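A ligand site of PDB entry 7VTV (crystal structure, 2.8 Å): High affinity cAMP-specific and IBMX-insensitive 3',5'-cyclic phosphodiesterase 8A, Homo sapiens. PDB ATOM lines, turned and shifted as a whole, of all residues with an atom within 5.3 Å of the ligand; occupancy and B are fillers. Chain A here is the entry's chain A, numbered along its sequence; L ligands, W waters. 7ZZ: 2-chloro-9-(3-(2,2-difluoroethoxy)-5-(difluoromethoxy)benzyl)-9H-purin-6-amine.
N7 of the ligand is in hydrogen-bond range of ND2 of Asn 248, at 3.0 Å.
The side-chain amide oxygen (OE1) of Gln 297 lies within hydrogen-bond range of a nitrogen (N6) of the ligand (3.1 Å).
A ring nitrogen (ND1) of His 192 sits at hydrogen-bond distance from the side-chain amino group (NZ) of Lys 242, at 3.3 Å.
The side-chain amide nitrogen (ND2) of Asn 248 is in hydrogen-bond range of the side-chain hydroxyl (OH) of Tyr 74 (3.1 Å).
A fluorine (FAU) of the ligand sits close to the backbone carbonyl oxygen (O) of Thr 187 (2.6 Å).
The backbone carbonyl oxygen (O) of Glu 188 sits close to a fluorine (FAU) of the ligand (3.1 Å).
A ring nitrogen (ND1) of His 192 lies close to a fluorine (FAV) of the ligand (3.1 Å).
Tyr 74 touches the ligand (OH to C8, 3.7 Å).
CG of Met 189 touches CAO of the ligand, at 3.3 Å.
Val 246 touches the ligand (CG1 to CAQ, 3.7 Å).
CG1 of Ile 263 touches C4 of the ligand, at 3.6 Å.
OH of Tyr 267 touches CAM of the ligand (3.2 Å).
Phe 286 touches the ligand (CE1 to FBA, 3.6 Å).
Phe 300 touches the ligand (CD1 to FAZ, 3.1 Å).
CE1 of Phe 304 touches FAZ of the ligand, at 3.4 Å.
Hydrophobic or aromatic side chains within 4 Å of the ligand: Met 189, His 192, Val 246, Ile 263, Tyr 267, Phe 286, Phe 300 and Phe 304.
13 residues have an atom within 4 Å of the ligand: Tyr 74, Thr 187, Glu 188, Met 189, His 192, Val 246, Asn 248, Ile 263, Tyr 267, Phe 286, Gln 297, Phe 300 and Phe 304.
The nearest printed residue that does not touch the ligand is Lys 242 (4.2 Å).
Water W1 bridges the backbone carbonyl oxygen (O) of Thr 187 (3.1 Å) and the side-chain carboxylate (OD2) of Asp 245 (3.1 Å).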
ATOM      1  N   TYR A  74     -28.299   0.966  -8.365  1.00  0.00           N
ATOM      2  CA  TYR A  74     -27.096   0.714  -9.154  1.00  0.00           C
ATOM      3  C   TYR A  74     -25.876   1.420  -8.549  1.00  0.00           C
ATOM      4  O   TYR A  74     -24.932   0.747  -8.128  1.00  0.00           O
ATOM      5  CB  TYR A  74     -27.298   1.180 -10.600  1.00  0.00           C
ATOM      6  CG  TYR A  74     -26.153   0.813 -11.517  1.00  0.00           C
ATOM      7  CD1 TYR A  74     -26.077  -0.459 -12.096  1.00  0.00           C
ATOM      8  CD2 TYR A  74     -25.147   1.729 -11.810  1.00  0.00           C
ATOM      9  CE1 TYR A  74     -25.031  -0.799 -12.949  1.00  0.00           C
ATOM     10  CE2 TYR A  74     -24.096   1.400 -12.641  1.00  0.00           C
ATOM     11  CZ  TYR A  74     -24.042   0.131 -13.216  1.00  0.00           C
ATOM     12  OH  TYR A  74     -23.000  -0.196 -14.051  1.00  0.00           O
ATOM     13  N   HIS A  75     -25.911   2.742  -8.497  1.00  0.00           N
ATOM     14  CA  HIS A  75     -24.739   3.554  -8.127  1.00  0.00           C
ATOM     15  C   HIS A  75     -24.484   3.523  -6.613  1.00  0.00           C
ATOM     16  O   HIS A  75     -24.763   4.498  -5.898  1.00  0.00           O
ATOM     17  CB  HIS A  75     -24.863   4.990  -8.645  1.00  0.00           C
ATOM     18  CG  HIS A  75     -24.578   5.122 -10.116  1.00  0.00           C
ATOM     19  ND1 HIS A  75     -25.554   5.329 -11.055  1.00  0.00           N
ATOM     20  CD2 HIS A  75     -23.409   5.066 -10.792  1.00  0.00           C
ATOM     21  CE1 HIS A  75     -25.008   5.404 -12.250  1.00  0.00           C
ATOM     22  NE2 HIS A  75     -23.702   5.239 -12.124  1.00  0.00           N
ATOM     23  N   ALA A 186     -13.015  11.323 -17.051  1.00  0.00           N
ATOM     24  CA  ALA A 186     -13.206  10.628 -18.335  1.00  0.00           C
ATOM     25  C   ALA A 186     -14.459   9.750 -18.406  1.00  0.00           C
ATOM     26  O   ALA A 186     -14.868   9.332 -19.491  1.00  0.00           O
ATOM     27  CB  ALA A 186     -11.990   9.798 -18.665  1.00  0.00           C
ATOM     28  N   THR A 187     -15.066   9.457 -17.254  1.00  0.00           N
ATOM     29  CA  THR A 187     -16.281   8.648 -17.177  1.00  0.00           C
ATOM     30  C   THR A 187     -17.579   9.399 -17.538  1.00  0.00           C
ATOM     31  O   THR A 187     -18.627   8.768 -17.625  1.00  0.00           O
ATOM     32  CB  THR A 187     -16.459   8.043 -15.766  1.00  0.00           C
ATOM     33  OG1 THR A 187     -16.573   9.091 -14.795  1.00  0.00           O
ATOM     34  CG2 THR A 187     -15.277   7.124 -15.417  1.00  0.00           C
ATOM     35  N   GLU A 188     -17.512  10.718 -17.739  1.00  0.00           N
ATOM     36  CA  GLU A 188     -18.682  11.524 -18.093  1.00  0.00           C
ATOM     37  C   GLU A 188     -19.339  11.035 -19.394  1.00  0.00           C
ATOM     38  O   GLU A 188     -18.649  10.639 -20.337  1.00  0.00           O
ATOM     39  CB  GLU A 188     -18.327  13.007 -18.224  1.00  0.00           C
ATOM     40  CG  GLU A 188     -19.537  13.941 -18.322  1.00  0.00           C
ATOM     41  CD  GLU A 188     -19.185  15.418 -18.297  1.00  0.00           C
ATOM     42  OE1 GLU A 188     -17.991  15.773 -18.263  1.00  0.00           O
ATOM     43  OE2 GLU A 188     -20.134  16.236 -18.320  1.00  0.00           O
ATOM     44  N   MET A 189     -20.674  11.081 -19.420  1.00  0.00           N
ATOM     45  CA  MET A 189     -21.464  10.534 -20.531  1.00  0.00           C
ATOM     46  C   MET A 189     -21.327  11.379 -21.794  1.00  0.00           C
ATOM     47  O   MET A 189     -21.220  10.836 -22.900  1.00  0.00           O
ATOM     48  CB  MET A 189     -22.938  10.411 -20.127  1.00  0.00           C
ATOM     49  CG  MET A 189     -23.742   9.406 -20.937  1.00  0.00           C
ATOM     50  SD  MET A 189     -24.505  10.044 -22.442  1.00  0.00           S
ATOM     51  CE  MET A 189     -25.839  11.010 -21.764  1.00  0.00           C
ATOM     52  N   HIS A 192     -18.392  10.779 -24.343  1.00  0.00           N
ATOM     53  CA  HIS A 192     -18.230   9.369 -24.757  1.00  0.00           C
ATOM     54  C   HIS A 192     -17.459   9.185 -26.058  1.00  0.00           C
ATOM     55  O   HIS A 192     -16.407   8.542 -26.080  1.00  0.00           O
ATOM     56  CB  HIS A 192     -19.596   8.682 -24.882  1.00  0.00           C
ATOM     57  CG  HIS A 192     -19.515   7.258 -25.348  1.00  0.00           C
ATOM     58  ND1 HIS A 192     -19.435   6.191 -24.479  1.00  0.00           N
ATOM     59  CD2 HIS A 192     -19.502   6.724 -26.596  1.00  0.00           C
ATOM     60  CE1 HIS A 192     -19.364   5.072 -25.172  1.00  0.00           C
ATOM     61  NE2 HIS A 192     -19.407   5.370 -26.461  1.00  0.00           N
ATOM     62  N   LYS A 242     -13.405   3.779 -18.921  1.00  0.00           N
ATOM     63  CA  LYS A 242     -14.694   3.821 -19.623  1.00  0.00           C
ATOM     64  C   LYS A 242     -15.282   2.425 -19.858  1.00  0.00           C
ATOM     65  O   LYS A 242     -16.478   2.229 -19.682  1.00  0.00           O
ATOM     66  CB  LYS A 242     -14.567   4.560 -20.960  1.00  0.00           C
ATOM     67  CG  LYS A 242     -14.583   6.078 -20.842  1.00  0.00           C
ATOM     68  CD  LYS A 242     -14.197   6.779 -22.145  1.00  0.00           C
ATOM     69  CE  LYS A 242     -15.138   6.418 -23.289  1.00  0.00           C
ATOM     70  NZ  LYS A 242     -16.561   6.648 -22.944  1.00  0.00           N
ATOM     71  N   ASP A 245     -16.131   0.783 -16.285  1.00  0.00           N
ATOM     72  CA  ASP A 245     -17.337   1.410 -15.729  1.00  0.00           C
ATOM     73  C   ASP A 245     -18.615   0.758 -16.262  1.00  0.00           C
ATOM     74  O   ASP A 245     -19.523   0.458 -15.483  1.00  0.00           O
ATOM     75  CB  ASP A 245     -17.360   2.913 -16.029  1.00  0.00           C
ATOM     76  CG  ASP A 245     -18.615   3.614 -15.495  1.00  0.00           C
ATOM     77  OD1 ASP A 245     -19.079   3.249 -14.390  1.00  0.00           O
ATOM     78  OD2 ASP A 245     -19.127   4.525 -16.182  1.00  0.00           O
ATOM     79  N   VAL A 246     -18.649   0.538 -17.571  1.00  0.00           N
ATOM     80  CA  VAL A 246     -19.841  -0.006 -18.260  1.00  0.00           C
ATOM     81  C   VAL A 246     -19.590  -1.435 -18.773  1.00  0.00           C
ATOM     82  O   VAL A 246     -19.999  -1.795 -19.875  1.00  0.00           O
ATOM     83  CB  VAL A 246     -20.339   0.937 -19.385  1.00  0.00           C
ATOM     84  CG1 VAL A 246     -20.747   2.280 -18.790  1.00  0.00           C
ATOM     85  CG2 VAL A 246     -19.305   1.142 -20.493  1.00  0.00           C
ATOM     86  N   ASN A 248     -20.858  -4.218 -17.516  1.00  0.00           N
ATOM     87  CA  ASN A 248     -21.954  -5.138 -17.163  1.00  0.00           C
ATOM     88  C   ASN A 248     -22.624  -5.907 -18.330  1.00  0.00           C
ATOM     89  O   ASN A 248     -23.025  -7.056 -18.147  1.00  0.00           O
ATOM     90  CB  ASN A 248     -23.008  -4.469 -16.248  1.00  0.00           C
ATOM     91  CG  ASN A 248     -23.744  -3.316 -16.910  1.00  0.00           C
ATOM     92  OD1 ASN A 248     -24.635  -3.523 -17.734  1.00  0.00           O
ATOM     93  ND2 ASN A 248     -23.393  -2.081 -16.522  1.00  0.00           N
ATOM     94  N   PRO A 249     -22.714  -5.293 -19.534  1.00  0.00           N
ATOM     95  CA  PRO A 249     -23.192  -6.072 -20.678  1.00  0.00           C
ATOM     96  C   PRO A 249     -22.226  -7.177 -21.138  1.00  0.00           C
ATOM     97  O   PRO A 249     -22.663  -8.131 -21.791  1.00  0.00           O
ATOM     98  CB  PRO A 249     -23.373  -5.014 -21.782  1.00  0.00           C
ATOM     99  CG  PRO A 249     -23.381  -3.707 -21.063  1.00  0.00           C
ATOM    100  CD  PRO A 249     -22.413  -3.919 -19.949  1.00  0.00           C
ATOM    101  N   TRP A 259     -27.548  -6.244 -13.105  1.00  0.00           N
ATOM    102  CA  TRP A 259     -27.094  -4.875 -13.363  1.00  0.00           C
ATOM    103  C   TRP A 259     -28.061  -4.088 -14.253  1.00  0.00           C
ATOM    104  O   TRP A 259     -28.186  -2.878 -14.107  1.00  0.00           O
ATOM    105  CB  TRP A 259     -25.688  -4.855 -14.003  1.00  0.00           C
ATOM    106  CG  TRP A 259     -24.546  -5.256 -13.090  1.00  0.00           C
ATOM    107  CD1 TRP A 259     -23.596  -6.209 -13.332  1.00  0.00           C
ATOM    108  CD2 TRP A 259     -24.231  -4.688 -11.808  1.00  0.00           C
ATOM    109  NE1 TRP A 259     -22.723  -6.283 -12.281  1.00  0.00           N
ATOM    110  CE2 TRP A 259     -23.074  -5.360 -11.328  1.00  0.00           C
ATOM    111  CE3 TRP A 259     -24.803  -3.691 -11.008  1.00  0.00           C
ATOM    112  CZ2 TRP A 259     -22.498  -5.070 -10.099  1.00  0.00           C
ATOM    113  CZ3 TRP A 259     -24.227  -3.401  -9.779  1.00  0.00           C
ATOM    114  CH2 TRP A 259     -23.083  -4.085  -9.333  1.00  0.00           C
ATOM    115  N   ALA A 260     -28.717  -4.778 -15.185  1.00  0.00           N
ATOM    116  CA  ALA A 260     -29.724  -4.168 -16.065  1.00  0.00           C
ATOM    117  C   ALA A 260     -30.948  -3.663 -15.302  1.00  0.00           C
ATOM    118  O   ALA A 260     -31.496  -2.605 -15.630  1.00  0.00           O
ATOM    119  CB  ALA A 260     -30.145  -5.151 -17.149  1.00  0.00           C
ATOM    120  N   ILE A 263     -29.791  -0.354 -12.728  1.00  0.00           N
ATOM    121  CA  ILE A 263     -29.680   0.902 -13.473  1.00  0.00           C
ATOM    122  C   ILE A 263     -31.038   1.369 -14.047  1.00  0.00           C
ATOM    123  O   ILE A 263     -31.301   2.577 -14.116  1.00  0.00           O
ATOM    124  CB  ILE A 263     -28.605   0.819 -14.599  1.00  0.00           C
ATOM    125  CG1 ILE A 263     -28.215   2.225 -15.098  1.00  0.00           C
ATOM    126  CG2 ILE A 263     -29.049  -0.067 -15.753  1.00  0.00           C
ATOM    127  CD1 ILE A 263     -27.243   2.955 -14.198  1.00  0.00           C
ATOM    128  N   TYR A 267     -33.287   4.832 -13.101  1.00  0.00           N
ATOM    129  CA  TYR A 267     -33.828   5.793 -14.073  1.00  0.00           C
ATOM    130  C   TYR A 267     -35.342   5.958 -14.017  1.00  0.00           C
ATOM    131  O   TYR A 267     -35.859   7.019 -14.378  1.00  0.00           O
ATOM    132  CB  TYR A 267     -33.400   5.436 -15.510  1.00  0.00           C
ATOM    133  CG  TYR A 267     -31.916   5.598 -15.791  1.00  0.00           C
ATOM    134  CD1 TYR A 267     -31.189   6.679 -15.272  1.00  0.00           C
ATOM    135  CD2 TYR A 267     -31.239   4.680 -16.603  1.00  0.00           C
ATOM    136  CE1 TYR A 267     -29.838   6.818 -15.535  1.00  0.00           C
ATOM    137  CE2 TYR A 267     -29.878   4.818 -16.863  1.00  0.00           C
ATOM    138  CZ  TYR A 267     -29.188   5.905 -16.323  1.00  0.00           C
ATOM    139  OH  TYR A 267     -27.853   6.079 -16.553  1.00  0.00           O
ATOM    140  N   PHE A 286     -37.047   5.979 -20.340  1.00  0.00           N
ATOM    141  CA  PHE A 286     -36.880   5.250 -19.080  1.00  0.00           C
ATOM    142  C   PHE A 286     -37.948   5.637 -18.062  1.00  0.00           C
ATOM    143  O   PHE A 286     -37.650   6.294 -17.057  1.00  0.00           O
ATOM    144  CB  PHE A 286     -35.479   5.487 -18.496  1.00  0.00           C
ATOM    145  CG  PHE A 286     -34.348   5.140 -19.429  1.00  0.00           C
ATOM    146  CD1 PHE A 286     -33.385   6.079 -19.746  1.00  0.00           C
ATOM    147  CD2 PHE A 286     -34.264   3.878 -19.996  1.00  0.00           C
ATOM    148  CE1 PHE A 286     -32.343   5.769 -20.614  1.00  0.00           C
ATOM    149  CE2 PHE A 286     -33.222   3.558 -20.863  1.00  0.00           C
ATOM    150  CZ  PHE A 286     -32.261   4.508 -21.172  1.00  0.00           C
ATOM    151  N   SER A 296     -34.468  -1.741 -24.372  1.00  0.00           N
ATOM    152  CA  SER A 296     -33.622  -0.639 -23.896  1.00  0.00           C
ATOM    153  C   SER A 296     -32.151  -1.046 -23.769  1.00  0.00           C
ATOM    154  O   SER A 296     -31.264  -0.249 -24.091  1.00  0.00           O
ATOM    155  CB  SER A 296     -34.132  -0.108 -22.554  1.00  0.00           C
ATOM    156  OG  SER A 296     -35.423   0.467 -22.705  1.00  0.00           O
ATOM    157  N   GLN A 297     -31.890  -2.259 -23.293  1.00  0.00           N
ATOM    158  CA  GLN A 297     -30.512  -2.779 -23.208  1.00  0.00           C
ATOM    159  C   GLN A 297     -29.875  -3.014 -24.571  1.00  0.00           C
ATOM    160  O   GLN A 297     -28.691  -2.756 -24.758  1.00  0.00           O
ATOM    161  CB  GLN A 297     -30.455  -4.069 -22.372  1.00  0.00           C
ATOM    162  CG  GLN A 297     -30.696  -3.870 -20.875  1.00  0.00           C
ATOM    163  CD  GLN A 297     -29.653  -2.997 -20.213  1.00  0.00           C
ATOM    164  OE1 GLN A 297     -28.526  -2.869 -20.682  1.00  0.00           O
ATOM    165  NE2 GLN A 297     -30.037  -2.370 -19.099  1.00  0.00           N
ATOM    166  N   PHE A 300     -28.942   0.471 -25.774  1.00  0.00           N
ATOM    167  CA  PHE A 300     -27.760   0.852 -24.995  1.00  0.00           C
ATOM    168  C   PHE A 300     -26.493   0.198 -25.552  1.00  0.00           C
ATOM    169  O   PHE A 300     -25.506   0.886 -25.822  1.00  0.00           O
ATOM    170  CB  PHE A 300     -27.935   0.475 -23.516  1.00  0.00           C
ATOM    171  CG  PHE A 300     -26.738   0.790 -22.663  1.00  0.00           C
ATOM    172  CD1 PHE A 300     -26.348   2.105 -22.462  1.00  0.00           C
ATOM    173  CD2 PHE A 300     -26.007  -0.225 -22.050  1.00  0.00           C
ATOM    174  CE1 PHE A 300     -25.236   2.404 -21.682  1.00  0.00           C
ATOM    175  CE2 PHE A 300     -24.905   0.075 -21.273  1.00  0.00           C
ATOM    176  CZ  PHE A 300     -24.521   1.390 -21.084  1.00  0.00           C
ATOM    177  N   PHE A 304     -23.588   2.630 -27.321  1.00  0.00           N
ATOM    178  CA  PHE A 304     -22.372   2.867 -26.526  1.00  0.00           C
ATOM    179  C   PHE A 304     -21.357   1.713 -26.549  1.00  0.00           C
ATOM    180  O   PHE A 304     -20.169   1.937 -26.762  1.00  0.00           O
ATOM    181  CB  PHE A 304     -22.757   3.121 -25.054  1.00  0.00           C
ATOM    182  CG  PHE A 304     -23.618   4.343 -24.851  1.00  0.00           C
ATOM    183  CD1 PHE A 304     -24.997   4.246 -24.841  1.00  0.00           C
ATOM    184  CD2 PHE A 304     -23.034   5.594 -24.652  1.00  0.00           C
ATOM    185  CE1 PHE A 304     -25.792   5.368 -24.649  1.00  0.00           C
ATOM    186  CE2 PHE A 304     -23.818   6.716 -24.457  1.00  0.00           C
ATOM    187  CZ  PHE A 304     -25.197   6.607 -24.456  1.00  0.00           C
HETATM  188  C2  7ZZ L   1     -28.123   1.736 -19.356  1.00  0.00           C
HETATM  189  C4  7ZZ L   1     -26.170   1.974 -18.109  1.00  0.00           C
HETATM  190  C5  7ZZ L   1     -26.005   0.641 -18.103  1.00  0.00           C
HETATM  191  C6  7ZZ L   1     -26.902  -0.125 -18.727  1.00  0.00           C
HETATM  192  N9  7ZZ L   1     -25.173   2.520 -17.431  1.00  0.00           N
HETATM  193  FAU 7ZZ L   1     -19.373   7.679 -19.912  1.00  0.00           F
HETATM  194  CAT 7ZZ L   1     -20.055   6.754 -20.687  1.00  0.00           C
HETATM  195  FAV 7ZZ L   1     -20.580   7.368 -21.791  1.00  0.00           F
HETATM  196  CAS 7ZZ L   1     -21.192   6.173 -19.855  1.00  0.00           C
HETATM  197  OAR 7ZZ L   1     -22.141   5.544 -20.728  1.00  0.00           O
HETATM  198  CAP 7ZZ L   1     -23.367   5.477 -20.148  1.00  0.00           C
HETATM  199  CAQ 7ZZ L   1     -23.554   4.752 -18.965  1.00  0.00           C
HETATM  200  CAO 7ZZ L   1     -24.444   6.141 -20.730  1.00  0.00           C
HETATM  201  CAN 7ZZ L   1     -25.710   6.089 -20.152  1.00  0.00           C
HETATM  202  OAW 7ZZ L   1     -26.740   6.768 -20.744  1.00  0.00           O
HETATM  203  CAY 7ZZ L   1     -27.882   6.033 -21.230  1.00  0.00           C
HETATM  204  FAZ 7ZZ L   1     -27.513   4.923 -21.759  1.00  0.00           F
HETATM  205  FBA 7ZZ L   1     -28.745   5.788 -20.227  1.00  0.00           F
HETATM  206  CAM 7ZZ L   1     -25.885   5.374 -18.967  1.00  0.00           C
HETATM  207  CAL 7ZZ L   1     -24.813   4.701 -18.374  1.00  0.00           C
HETATM  208  CAK 7ZZ L   1     -24.973   3.974 -17.174  1.00  0.00           C
HETATM  209  C8  7ZZ L   1     -24.385   1.533 -17.004  1.00  0.00           C
HETATM  210  N7  7ZZ L   1     -24.897   0.376 -17.424  1.00  0.00           N
HETATM  211  N3  7ZZ L   1     -27.236   2.523 -18.727  1.00  0.00           N
HETATM  212 CL2  7ZZ L   1     -29.450   2.463 -20.139  1.00  0.00          CL
HETATM  213  N1  7ZZ L   1     -27.956   0.401 -19.360  1.00  0.00           N
HETATM  214  N6  7ZZ L   1     -26.679  -1.432 -18.699  1.00  0.00           N
HETATM  215  O   HOH W   1     -17.812   5.935 -18.641  1.00  0.00           O
